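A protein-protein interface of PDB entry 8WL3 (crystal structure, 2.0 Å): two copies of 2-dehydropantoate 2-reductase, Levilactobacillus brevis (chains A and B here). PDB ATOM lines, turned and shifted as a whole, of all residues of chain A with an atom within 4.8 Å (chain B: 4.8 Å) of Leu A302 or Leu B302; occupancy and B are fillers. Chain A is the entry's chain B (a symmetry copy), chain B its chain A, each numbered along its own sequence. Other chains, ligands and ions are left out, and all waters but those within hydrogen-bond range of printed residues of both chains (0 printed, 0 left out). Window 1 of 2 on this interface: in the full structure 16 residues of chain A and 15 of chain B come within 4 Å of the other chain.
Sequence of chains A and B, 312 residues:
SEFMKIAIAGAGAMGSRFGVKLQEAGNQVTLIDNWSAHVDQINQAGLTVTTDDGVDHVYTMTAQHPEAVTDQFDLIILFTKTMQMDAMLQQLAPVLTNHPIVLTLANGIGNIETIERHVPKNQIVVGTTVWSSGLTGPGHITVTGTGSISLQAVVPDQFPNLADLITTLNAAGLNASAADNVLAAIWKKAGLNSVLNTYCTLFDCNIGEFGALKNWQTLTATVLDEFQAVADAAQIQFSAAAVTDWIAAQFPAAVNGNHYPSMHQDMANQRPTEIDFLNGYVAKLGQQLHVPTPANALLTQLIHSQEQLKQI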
ATOM      1  N   TYR A 199     -28.179  11.529  -1.052  1.00  0.00           N
ATOM      2  CA  TYR A 199     -27.523  10.440  -0.323  1.00  0.00           C
ATOM      3  C   TYR A 199     -28.100   9.068  -0.690  1.00  0.00           C
ATOM      4  O   TYR A 199     -27.354   8.082  -0.820  1.00  0.00           O
ATOM      5  CB  TYR A 199     -27.617  10.654   1.174  1.00  0.00           C
ATOM      6  CG  TYR A 199     -26.654  11.696   1.737  1.00  0.00           C
ATOM      7  CD1 TYR A 199     -25.277  11.604   1.527  1.00  0.00           C
ATOM      8  CD2 TYR A 199     -27.115  12.764   2.510  1.00  0.00           C
ATOM      9  CE1 TYR A 199     -24.393  12.542   2.084  1.00  0.00           C
ATOM     10  CE2 TYR A 199     -26.235  13.682   3.068  1.00  0.00           C
ATOM     11  CZ  TYR A 199     -24.877  13.553   2.859  1.00  0.00           C
ATOM     12  OH  TYR A 199     -23.997  14.490   3.412  1.00  0.00           O
ATOM     13  N   LEU A 202     -26.427   8.193  -3.965  1.00  0.00           N
ATOM     14  CA  LEU A 202     -25.038   7.779  -3.780  1.00  0.00           C
ATOM     15  C   LEU A 202     -24.895   6.414  -3.129  1.00  0.00           C
ATOM     16  O   LEU A 202     -23.971   5.703  -3.437  1.00  0.00           O
ATOM     17  CB  LEU A 202     -24.278   8.770  -2.908  1.00  0.00           C
ATOM     18  CG  LEU A 202     -24.011  10.140  -3.512  1.00  0.00           C
ATOM     19  CD1 LEU A 202     -23.503  11.138  -2.464  1.00  0.00           C
ATOM     20  CD2 LEU A 202     -22.995   9.980  -4.635  1.00  0.00           C
ATOM     21  N   PHE A 203     -25.763   6.099  -2.180  1.00  0.00           N
ATOM     22  CA  PHE A 203     -25.676   4.874  -1.396  1.00  0.00           C
ATOM     23  C   PHE A 203     -26.542   3.739  -1.966  1.00  0.00           C
ATOM     24  O   PHE A 203     -26.533   2.630  -1.406  1.00  0.00           O
ATOM     25  CB  PHE A 203     -26.160   5.132   0.050  1.00  0.00           C
ATOM     26  CG  PHE A 203     -25.319   6.111   0.844  1.00  0.00           C
ATOM     27  CD1 PHE A 203     -23.940   6.195   0.680  1.00  0.00           C
ATOM     28  CD2 PHE A 203     -25.917   6.913   1.801  1.00  0.00           C
ATOM     29  CE1 PHE A 203     -23.187   7.076   1.448  1.00  0.00           C
ATOM     30  CE2 PHE A 203     -25.171   7.797   2.573  1.00  0.00           C
ATOM     31  CZ  PHE A 203     -23.806   7.878   2.408  1.00  0.00           C
ATOM     32  N   LEU A 219     -24.131  13.453   8.314  1.00  0.00           N
ATOM     33  CA  LEU A 219     -24.302  13.640   6.869  1.00  0.00           C
ATOM     34  C   LEU A 219     -25.304  14.779   6.575  1.00  0.00           C
ATOM     35  O   LEU A 219     -25.069  15.633   5.710  1.00  0.00           O
ATOM     36  CB  LEU A 219     -24.790  12.338   6.213  1.00  0.00           C
ATOM     37  CG  LEU A 219     -23.856  11.135   6.174  1.00  0.00           C
ATOM     38  CD1 LEU A 219     -24.622   9.943   5.587  1.00  0.00           C
ATOM     39  CD2 LEU A 219     -22.601  11.428   5.345  1.00  0.00           C
ATOM     40  N   LEU A 298     -18.630  18.863  -3.627  1.00  0.00           N
ATOM     41  CA  LEU A 298     -18.138  17.495  -3.777  1.00  0.00           C
ATOM     42  C   LEU A 298     -19.286  16.523  -4.047  1.00  0.00           C
ATOM     43  O   LEU A 298     -19.177  15.704  -4.962  1.00  0.00           O
ATOM     44  CB  LEU A 298     -17.350  17.054  -2.550  1.00  0.00           C
ATOM     45  CG  LEU A 298     -16.786  15.632  -2.547  1.00  0.00           C
ATOM     46  CD1 LEU A 298     -15.831  15.439  -3.691  1.00  0.00           C
ATOM     47  CD2 LEU A 298     -16.084  15.364  -1.216  1.00  0.00           C
ATOM     48  N   LEU A 299     -20.384  16.621  -3.279  1.00  0.00           N
ATOM     49  CA  LEU A 299     -21.510  15.714  -3.500  1.00  0.00           C
ATOM     50  C   LEU A 299     -22.014  15.844  -4.926  1.00  0.00           C
ATOM     51  O   LEU A 299     -22.369  14.849  -5.541  1.00  0.00           O
ATOM     52  CB  LEU A 299     -22.669  15.915  -2.495  1.00  0.00           C
ATOM     53  CG  LEU A 299     -22.311  15.568  -1.061  1.00  0.00           C
ATOM     54  CD1 LEU A 299     -23.376  16.152  -0.128  1.00  0.00           C
ATOM     55  CD2 LEU A 299     -22.096  14.056  -0.860  1.00  0.00           C
ATOM     56  N   THR A 300     -22.023  17.069  -5.441  1.00  0.00           N
ATOM     57  CA  THR A 300     -22.442  17.327  -6.815  1.00  0.00           C
ATOM     58  C   THR A 300     -21.517  16.585  -7.812  1.00  0.00           C
ATOM     59  O   THR A 300     -21.984  15.940  -8.744  1.00  0.00           O
ATOM     60  CB  THR A 300     -22.491  18.848  -7.078  1.00  0.00           C
ATOM     61  OG1 THR A 300     -23.459  19.449  -6.187  1.00  0.00           O
ATOM     62  CG2 THR A 300     -22.857  19.180  -8.521  1.00  0.00           C
ATOM     63  N   GLN A 301     -20.217  16.657  -7.594  1.00  0.00           N
ATOM     64  CA  GLN A 301     -19.260  15.981  -8.449  1.00  0.00           C
ATOM     65  C   GLN A 301     -19.431  14.459  -8.420  1.00  0.00           C
ATOM     66  O   GLN A 301     -19.349  13.794  -9.475  1.00  0.00           O
ATOM     67  CB  GLN A 301     -17.832  16.350  -8.047  1.00  0.00           C
ATOM     68  CG  GLN A 301     -17.459  17.799  -8.310  1.00  0.00           C
ATOM     69  CD  GLN A 301     -17.520  18.153  -9.788  1.00  0.00           C
ATOM     70  OE1 GLN A 301     -17.119  17.367 -10.633  1.00  0.00           O
ATOM     71  NE2 GLN A 301     -18.044  19.338 -10.105  1.00  0.00           N
ATOM     72  N   LEU A 302     -19.685  13.922  -7.230  1.00  0.00           N
ATOM     73  CA  LEU A 302     -19.852  12.481  -7.057  1.00  0.00           C
ATOM     74  C   LEU A 302     -21.052  11.989  -7.841  1.00  0.00           C
ATOM     75  O   LEU A 302     -20.999  10.936  -8.481  1.00  0.00           O
ATOM     76  CB  LEU A 302     -19.991  12.102  -5.570  1.00  0.00           C
ATOM     77  CG  LEU A 302     -18.850  12.436  -4.597  1.00  0.00           C
ATOM     78  CD1 LEU A 302     -19.243  12.083  -3.159  1.00  0.00           C
ATOM     79  CD2 LEU A 302     -17.545  11.748  -4.996  1.00  0.00           C
ATOM     80  N   ILE A 303     -22.141  12.757  -7.783  1.00  0.00           N
ATOM     81  CA  ILE A 303     -23.355  12.419  -8.532  1.00  0.00           C
ATOM     82  C   ILE A 303     -23.113  12.473 -10.053  1.00  0.00           C
ATOM     83  O   ILE A 303     -23.509  11.557 -10.783  1.00  0.00           O
ATOM     84  CB  ILE A 303     -24.552  13.311  -8.128  1.00  0.00           C
ATOM     85  CG1 ILE A 303     -25.064  12.946  -6.728  1.00  0.00           C
ATOM     86  CG2 ILE A 303     -25.706  13.159  -9.118  1.00  0.00           C
ATOM     87  CD1 ILE A 303     -25.679  11.557  -6.577  1.00  0.00           C
ATOM     88  N   HIS A 304     -22.464  13.538 -10.533  1.00  0.00           N
ATOM     89  CA  HIS A 304     -22.064  13.606 -11.945  1.00  0.00           C
ATOM     90  C   HIS A 304     -21.206  12.400 -12.395  1.00  0.00           C
ATOM     91  O   HIS A 304     -21.444  11.842 -13.475  1.00  0.00           O
ATOM     92  CB  HIS A 304     -21.366  14.941 -12.240  1.00  0.00           C
ATOM     93  CG  HIS A 304     -22.309  16.101 -12.305  1.00  0.00           C
ATOM     94  ND1 HIS A 304     -23.526  16.023 -12.950  1.00  0.00           N
ATOM     95  CD2 HIS A 304     -22.219  17.364 -11.828  1.00  0.00           C
ATOM     96  CE1 HIS A 304     -24.158  17.178 -12.841  1.00  0.00           C
ATOM     97  NE2 HIS A 304     -23.382  18.014 -12.169  1.00  0.00           N
ATOM     98  N   SER A 305     -20.265  11.955 -11.557  1.00  0.00           N
ATOM     99  CA  SER A 305     -19.452  10.792 -11.895  1.00  0.00           C
ATOM    100  C   SER A 305     -20.290   9.536 -11.968  1.00  0.00           C
ATOM    101  O   SER A 305     -20.117   8.698 -12.857  1.00  0.00           O
ATOM    102  CB  SER A 305     -18.333  10.601 -10.877  1.00  0.00           C
ATOM    103  OG  SER A 305     -17.460  11.707 -10.887  1.00  0.00           O
ATOM    104  N   GLN A 306     -21.183   9.378 -11.000  1.00  0.00           N
ATOM    105  CA  GLN A 306     -22.076   8.227 -10.977  1.00  0.00           C
ATOM    106  C   GLN A 306     -22.937   8.199 -12.261  1.00  0.00           C
ATOM    107  O   GLN A 306     -23.121   7.151 -12.874  1.00  0.00           O
ATOM    108  CB  GLN A 306     -22.945   8.289  -9.710  1.00  0.00           C
ATOM    109  CG  GLN A 306     -23.603   6.991  -9.291  1.00  0.00           C
ATOM    110  CD  GLN A 306     -24.482   7.185  -8.055  1.00  0.00           C
ATOM    111  OE1 GLN A 306     -24.278   8.127  -7.270  1.00  0.00           O
ATOM    112  NE2 GLN A 306     -25.466   6.319  -7.884  1.00  0.00           N
ATOM    113  N   TYR B 199     -12.435   6.581  -4.094  1.00  0.00           N
ATOM    114  CA  TYR B 199     -13.373   6.891  -5.165  1.00  0.00           C
ATOM    115  C   TYR B 199     -13.853   5.642  -5.920  1.00  0.00           C
ATOM    116  O   TYR B 199     -15.043   5.508  -6.261  1.00  0.00           O
ATOM    117  CB  TYR B 199     -12.789   7.889  -6.142  1.00  0.00           C
ATOM    118  CG  TYR B 199     -12.749   9.331  -5.635  1.00  0.00           C
ATOM    119  CD1 TYR B 199     -13.899   9.980  -5.209  1.00  0.00           C
ATOM    120  CD2 TYR B 199     -11.560  10.059  -5.651  1.00  0.00           C
ATOM    121  CE1 TYR B 199     -13.856  11.306  -4.767  1.00  0.00           C
ATOM    122  CE2 TYR B 199     -11.512  11.372  -5.235  1.00  0.00           C
ATOM    123  CZ  TYR B 199     -12.669  12.002  -4.799  1.00  0.00           C
ATOM    124  OH  TYR B 199     -12.618  13.334  -4.399  1.00  0.00           O
ATOM    125  N   LEU B 202     -16.524   4.121  -3.679  1.00  0.00           N
ATOM    126  CA  LEU B 202     -17.789   4.862  -3.741  1.00  0.00           C
ATOM    127  C   LEU B 202     -18.512   4.682  -5.058  1.00  0.00           C
ATOM    128  O   LEU B 202     -19.735   4.666  -5.092  1.00  0.00           O
ATOM    129  CB  LEU B 202     -17.563   6.369  -3.568  1.00  0.00           C
ATOM    130  CG  LEU B 202     -17.118   6.799  -2.166  1.00  0.00           C
ATOM    131  CD1 LEU B 202     -16.635   8.245  -2.121  1.00  0.00           C
ATOM    132  CD2 LEU B 202     -18.273   6.585  -1.188  1.00  0.00           C
ATOM    133  N   PHE B 203     -17.763   4.613  -6.159  1.00  0.00           N
ATOM    134  CA  PHE B 203     -18.359   4.568  -7.481  1.00  0.00           C
ATOM    135  C   PHE B 203     -18.523   3.120  -7.989  1.00  0.00           C
ATOM    136  O   PHE B 203     -19.069   2.934  -9.050  1.00  0.00           O
ATOM    137  CB  PHE B 203     -17.480   5.323  -8.503  1.00  0.00           C
ATOM    138  CG  PHE B 203     -17.324   6.801  -8.254  1.00  0.00           C
ATOM    139  CD1 PHE B 203     -18.366   7.568  -7.755  1.00  0.00           C
ATOM    140  CD2 PHE B 203     -16.140   7.442  -8.586  1.00  0.00           C
ATOM    141  CE1 PHE B 203     -18.218   8.930  -7.564  1.00  0.00           C
ATOM    142  CE2 PHE B 203     -15.993   8.806  -8.398  1.00  0.00           C
ATOM    143  CZ  PHE B 203     -17.034   9.546  -7.875  1.00  0.00           C
ATOM    144  N   LEU B 219     -11.912  15.824  -8.697  1.00  0.00           N
ATOM    145  CA  LEU B 219     -12.028  14.887  -7.567  1.00  0.00           C
ATOM    146  C   LEU B 219     -10.663  14.635  -6.902  1.00  0.00           C
ATOM    147  O   LEU B 219     -10.536  14.636  -5.661  1.00  0.00           O
ATOM    148  CB  LEU B 219     -12.653  13.567  -8.034  1.00  0.00           C
ATOM    149  CG  LEU B 219     -14.102  13.561  -8.488  1.00  0.00           C
ATOM    150  CD1 LEU B 219     -14.481  12.195  -9.037  1.00  0.00           C
ATOM    151  CD2 LEU B 219     -15.047  13.908  -7.345  1.00  0.00           C
ATOM    152  N   LEU B 298     -15.819  14.198   4.905  1.00  0.00           N
ATOM    153  CA  LEU B 298     -17.054  13.728   4.289  1.00  0.00           C
ATOM    154  C   LEU B 298     -16.830  12.390   3.574  1.00  0.00           C
ATOM    155  O   LEU B 298     -17.639  11.470   3.735  1.00  0.00           O
ATOM    156  CB  LEU B 298     -17.622  14.762   3.321  1.00  0.00           C
ATOM    157  CG  LEU B 298     -18.947  14.368   2.626  1.00  0.00           C
ATOM    158  CD1 LEU B 298     -20.046  14.051   3.612  1.00  0.00           C
ATOM    159  CD2 LEU B 298     -19.437  15.456   1.685  1.00  0.00           C
ATOM    160  N   LEU B 299     -15.752  12.277   2.788  1.00  0.00           N
ATOM    161  CA  LEU B 299     -15.473  11.013   2.099  1.00  0.00           C
ATOM    162  C   LEU B 299     -15.383   9.871   3.101  1.00  0.00           C
ATOM    163  O   LEU B 299     -15.893   8.784   2.818  1.00  0.00           O
ATOM    164  CB  LEU B 299     -14.217  11.075   1.234  1.00  0.00           C
ATOM    165  CG  LEU B 299     -14.338  11.988   0.001  1.00  0.00           C
ATOM    166  CD1 LEU B 299     -12.981  12.227  -0.618  1.00  0.00           C
ATOM    167  CD2 LEU B 299     -15.274  11.413  -1.042  1.00  0.00           C
ATOM    168  N   THR B 300     -14.793  10.139   4.266  1.00  0.00           N
ATOM    169  CA  THR B 300     -14.688   9.155   5.330  1.00  0.00           C
ATOM    170  C   THR B 300     -16.091   8.692   5.788  1.00  0.00           C
ATOM    171  O   THR B 300     -16.362   7.502   5.921  1.00  0.00           O
ATOM    172  CB  THR B 300     -13.847   9.708   6.510  1.00  0.00           C
ATOM    173  OG1 THR B 300     -12.523  10.037   6.055  1.00  0.00           O
ATOM    174  CG2 THR B 300     -13.747   8.707   7.659  1.00  0.00           C
ATOM    175  N   GLN B 301     -16.980   9.647   6.000  1.00  0.00           N
ATOM    176  CA  GLN B 301     -18.333   9.356   6.437  1.00  0.00           C
ATOM    177  C   GLN B 301     -19.107   8.541   5.395  1.00  0.00           C
ATOM    178  O   GLN B 301     -19.865   7.620   5.748  1.00  0.00           O
ATOM    179  CB  GLN B 301     -19.076  10.649   6.725  1.00  0.00           C
ATOM    180  CG  GLN B 301     -18.580  11.418   7.948  1.00  0.00           C
ATOM    181  CD  GLN B 301     -18.695  10.612   9.225  1.00  0.00           C
ATOM    182  OE1 GLN B 301     -19.644   9.872   9.423  1.00  0.00           O
ATOM    183  NE2 GLN B 301     -17.698  10.733  10.084  1.00  0.00           N
ATOM    184  N   LEU B 302     -18.919   8.879   4.121  1.00  0.00           N
ATOM    185  CA  LEU B 302     -19.619   8.199   3.034  1.00  0.00           C
ATOM    186  C   LEU B 302     -19.224   6.735   2.991  1.00  0.00           C
ATOM    187  O   LEU B 302     -20.077   5.864   2.778  1.00  0.00           O
ATOM    188  CB  LEU B 302     -19.327   8.863   1.676  1.00  0.00           C
ATOM    189  CG  LEU B 302     -19.777  10.310   1.458  1.00  0.00           C
ATOM    190  CD1 LEU B 302     -19.365  10.796   0.083  1.00  0.00           C
ATOM    191  CD2 LEU B 302     -21.285  10.436   1.603  1.00  0.00           C
ATOM    192  N   ILE B 303     -17.931   6.483   3.179  1.00  0.00           N
ATOM    193  CA  ILE B 303     -17.416   5.116   3.164  1.00  0.00           C
ATOM    194  C   ILE B 303     -17.966   4.328   4.380  1.00  0.00           C
ATOM    195  O   ILE B 303     -18.412   3.191   4.232  1.00  0.00           O
ATOM    196  CB  ILE B 303     -15.861   5.088   3.119  1.00  0.00           C
ATOM    197  CG1 ILE B 303     -15.351   5.491   1.734  1.00  0.00           C
ATOM    198  CG2 ILE B 303     -15.334   3.689   3.446  1.00  0.00           C
ATOM    199  CD1 ILE B 303     -15.745   4.572   0.571  1.00  0.00           C
ATOM    200  N   HIS B 304     -17.953   4.945   5.565  1.00  0.00           N
ATOM    201  CA  HIS B 304     -18.610   4.337   6.732  1.00  0.00           C
ATOM    202  C   HIS B 304     -20.092   3.974   6.499  1.00  0.00           C
ATOM    203  O   HIS B 304     -20.524   2.864   6.859  1.00  0.00           O
ATOM    204  CB  HIS B 304     -18.416   5.196   7.995  1.00  0.00           C
ATOM    205  CG  HIS B 304     -17.023   5.147   8.540  1.00  0.00           C
ATOM    206  ND1 HIS B 304     -16.299   3.972   8.616  1.00  0.00           N
ATOM    207  CD2 HIS B 304     -16.218   6.112   9.033  1.00  0.00           C
ATOM    208  CE1 HIS B 304     -15.116   4.214   9.152  1.00  0.00           C
ATOM    209  NE2 HIS B 304     -15.032   5.509   9.401  1.00  0.00           N
ATOM    210  N   SER B 305     -20.857   4.869   5.858  1.00  0.00           N
ATOM    211  CA  SER B 305     -22.266   4.567   5.563  1.00  0.00           C
ATOM    212  C   SER B 305     -22.380   3.402   4.589  1.00  0.00           C
ATOM    213  O   SER B 305     -23.249   2.516   4.739  1.00  0.00           O
ATOM    214  CB  SER B 305     -22.972   5.792   4.972  1.00  0.00           C
ATOM    215  OG  SER B 305     -22.954   6.847   5.898  1.00  0.00           O
ATOM    216  N   GLN B 306     -21.523   3.403   3.574  1.00  0.00           N
ATOM    217  CA  GLN B 306     -21.528   2.330   2.593  1.00  0.00           C
ATOM    218  C   GLN B 306     -21.226   0.969   3.278  1.00  0.00           C
ATOM    219  O   GLN B 306     -21.885  -0.038   2.982  1.00  0.00           O
ATOM    220  CB  GLN B 306     -20.516   2.641   1.486  1.00  0.00           C
ATOM    221  CG  GLN B 306     -20.698   1.860   0.201  1.00  0.00           C
ATOM    222  CD  GLN B 306     -19.641   2.209  -0.840  1.00  0.00           C
ATOM    223  OE1 GLN B 306     -19.058   3.273  -0.788  1.00  0.00           O
ATOM    224  NE2 GLN B 306     -19.362   1.279  -1.751  1.00  0.00           N
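The backbone carbonyl oxygen (O) of Gln A301 is in hydrogen-bond range of the side-chain hydroxyl (OG) of Ser A305 (3.1 Å). OH of Tyr B199 sits at hydrogen-bond distance from O of Leu B219 (2.8 Å). O of Gln B301 is in hydrogen-bond range of OG of Ser B305, 3.2 Å away. The side-chain hydroxyl of Tyr A199 lies within hydrogen-bond range of the backbone carbonyl oxygen of Leu A219 (2.8 Å).
Tyr A199 touches Leu B298, and with the chains exchanged Leu A298 touches Tyr B199. Tyr A199 touches Leu B302, and with the chains exchanged Leu A302 touches Tyr B199. Leu A219 touches Ser B305, and with the chains exchanged Ser A305 touches Leu B219. Leu A298 touches Leu B299, and with the chains exchanged Leu A299 touches Leu B298. Of the 15 pairs that touch across the chains among the printed residues, 15 have their exchanged pair printed and touching as well.
Along chain B the printed residues that touch a printed residue of chain A span positions 199 to 305. Of the 13 printed residues of chain A, 8 touch a printed residue of chain B. Printed residues of chain A that touch a printed residue of chain B: Tyr A199, Phe A203, Leu A219, Leu A298, Leu A299, Gln A301, Leu A302 and Ser A305. Among the printed residues, 15 pairs touch across the chains.
Printed residues of chain B within 4 Å of Leu A219: Gln B301 (3.9 Å) and Ser B305 (3.5 Å). Of the printed residues of chain B, Gln A301 touches Leu B219 (3.8 Å). Leu A302 touches just these residues of chain B: Tyr B199 (3.7 Å), Phe B203 (3.5 Å) and Leu B302 (3.5 Å). Of the printed residues of chain B, Ser A305 touches Phe B203 (3.4 Å) and Leu B219 (3.5 Å). Of the printed residues of chain A, Tyr B199 touches Leu A298 and Leu A302. Of the printed residues of chain A, Leu B298 touches Tyr A199 (3.98 Å) and Leu A299 (3.9 Å). Thr B300 touches none of the printed residues of chain A. Printed residues of chain A within 4 Å of Leu B302: Tyr A199, Phe A203 and Leu A302. Gln B306 touches none of the printed residues of chain A.
Tyr A199 touches Leu B298. Gln B301 touches Leu A219. OG of Ser B305 touches CD1 of Leu A219, 3.5 Å away. Leu A298 touches Tyr B199. Leu B299 touches Leu A298 (CG to CD2, 3.99 Å). Gln A301 touches Leu B219 (CB to CD2, 3.8 Å). Tyr B199 touches Leu A302. Leu A302 touches Phe B203. CD1 of Leu A302 touches CD1 of Leu B302, 3.5 Å away. Ser A305 touches Leu B219.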
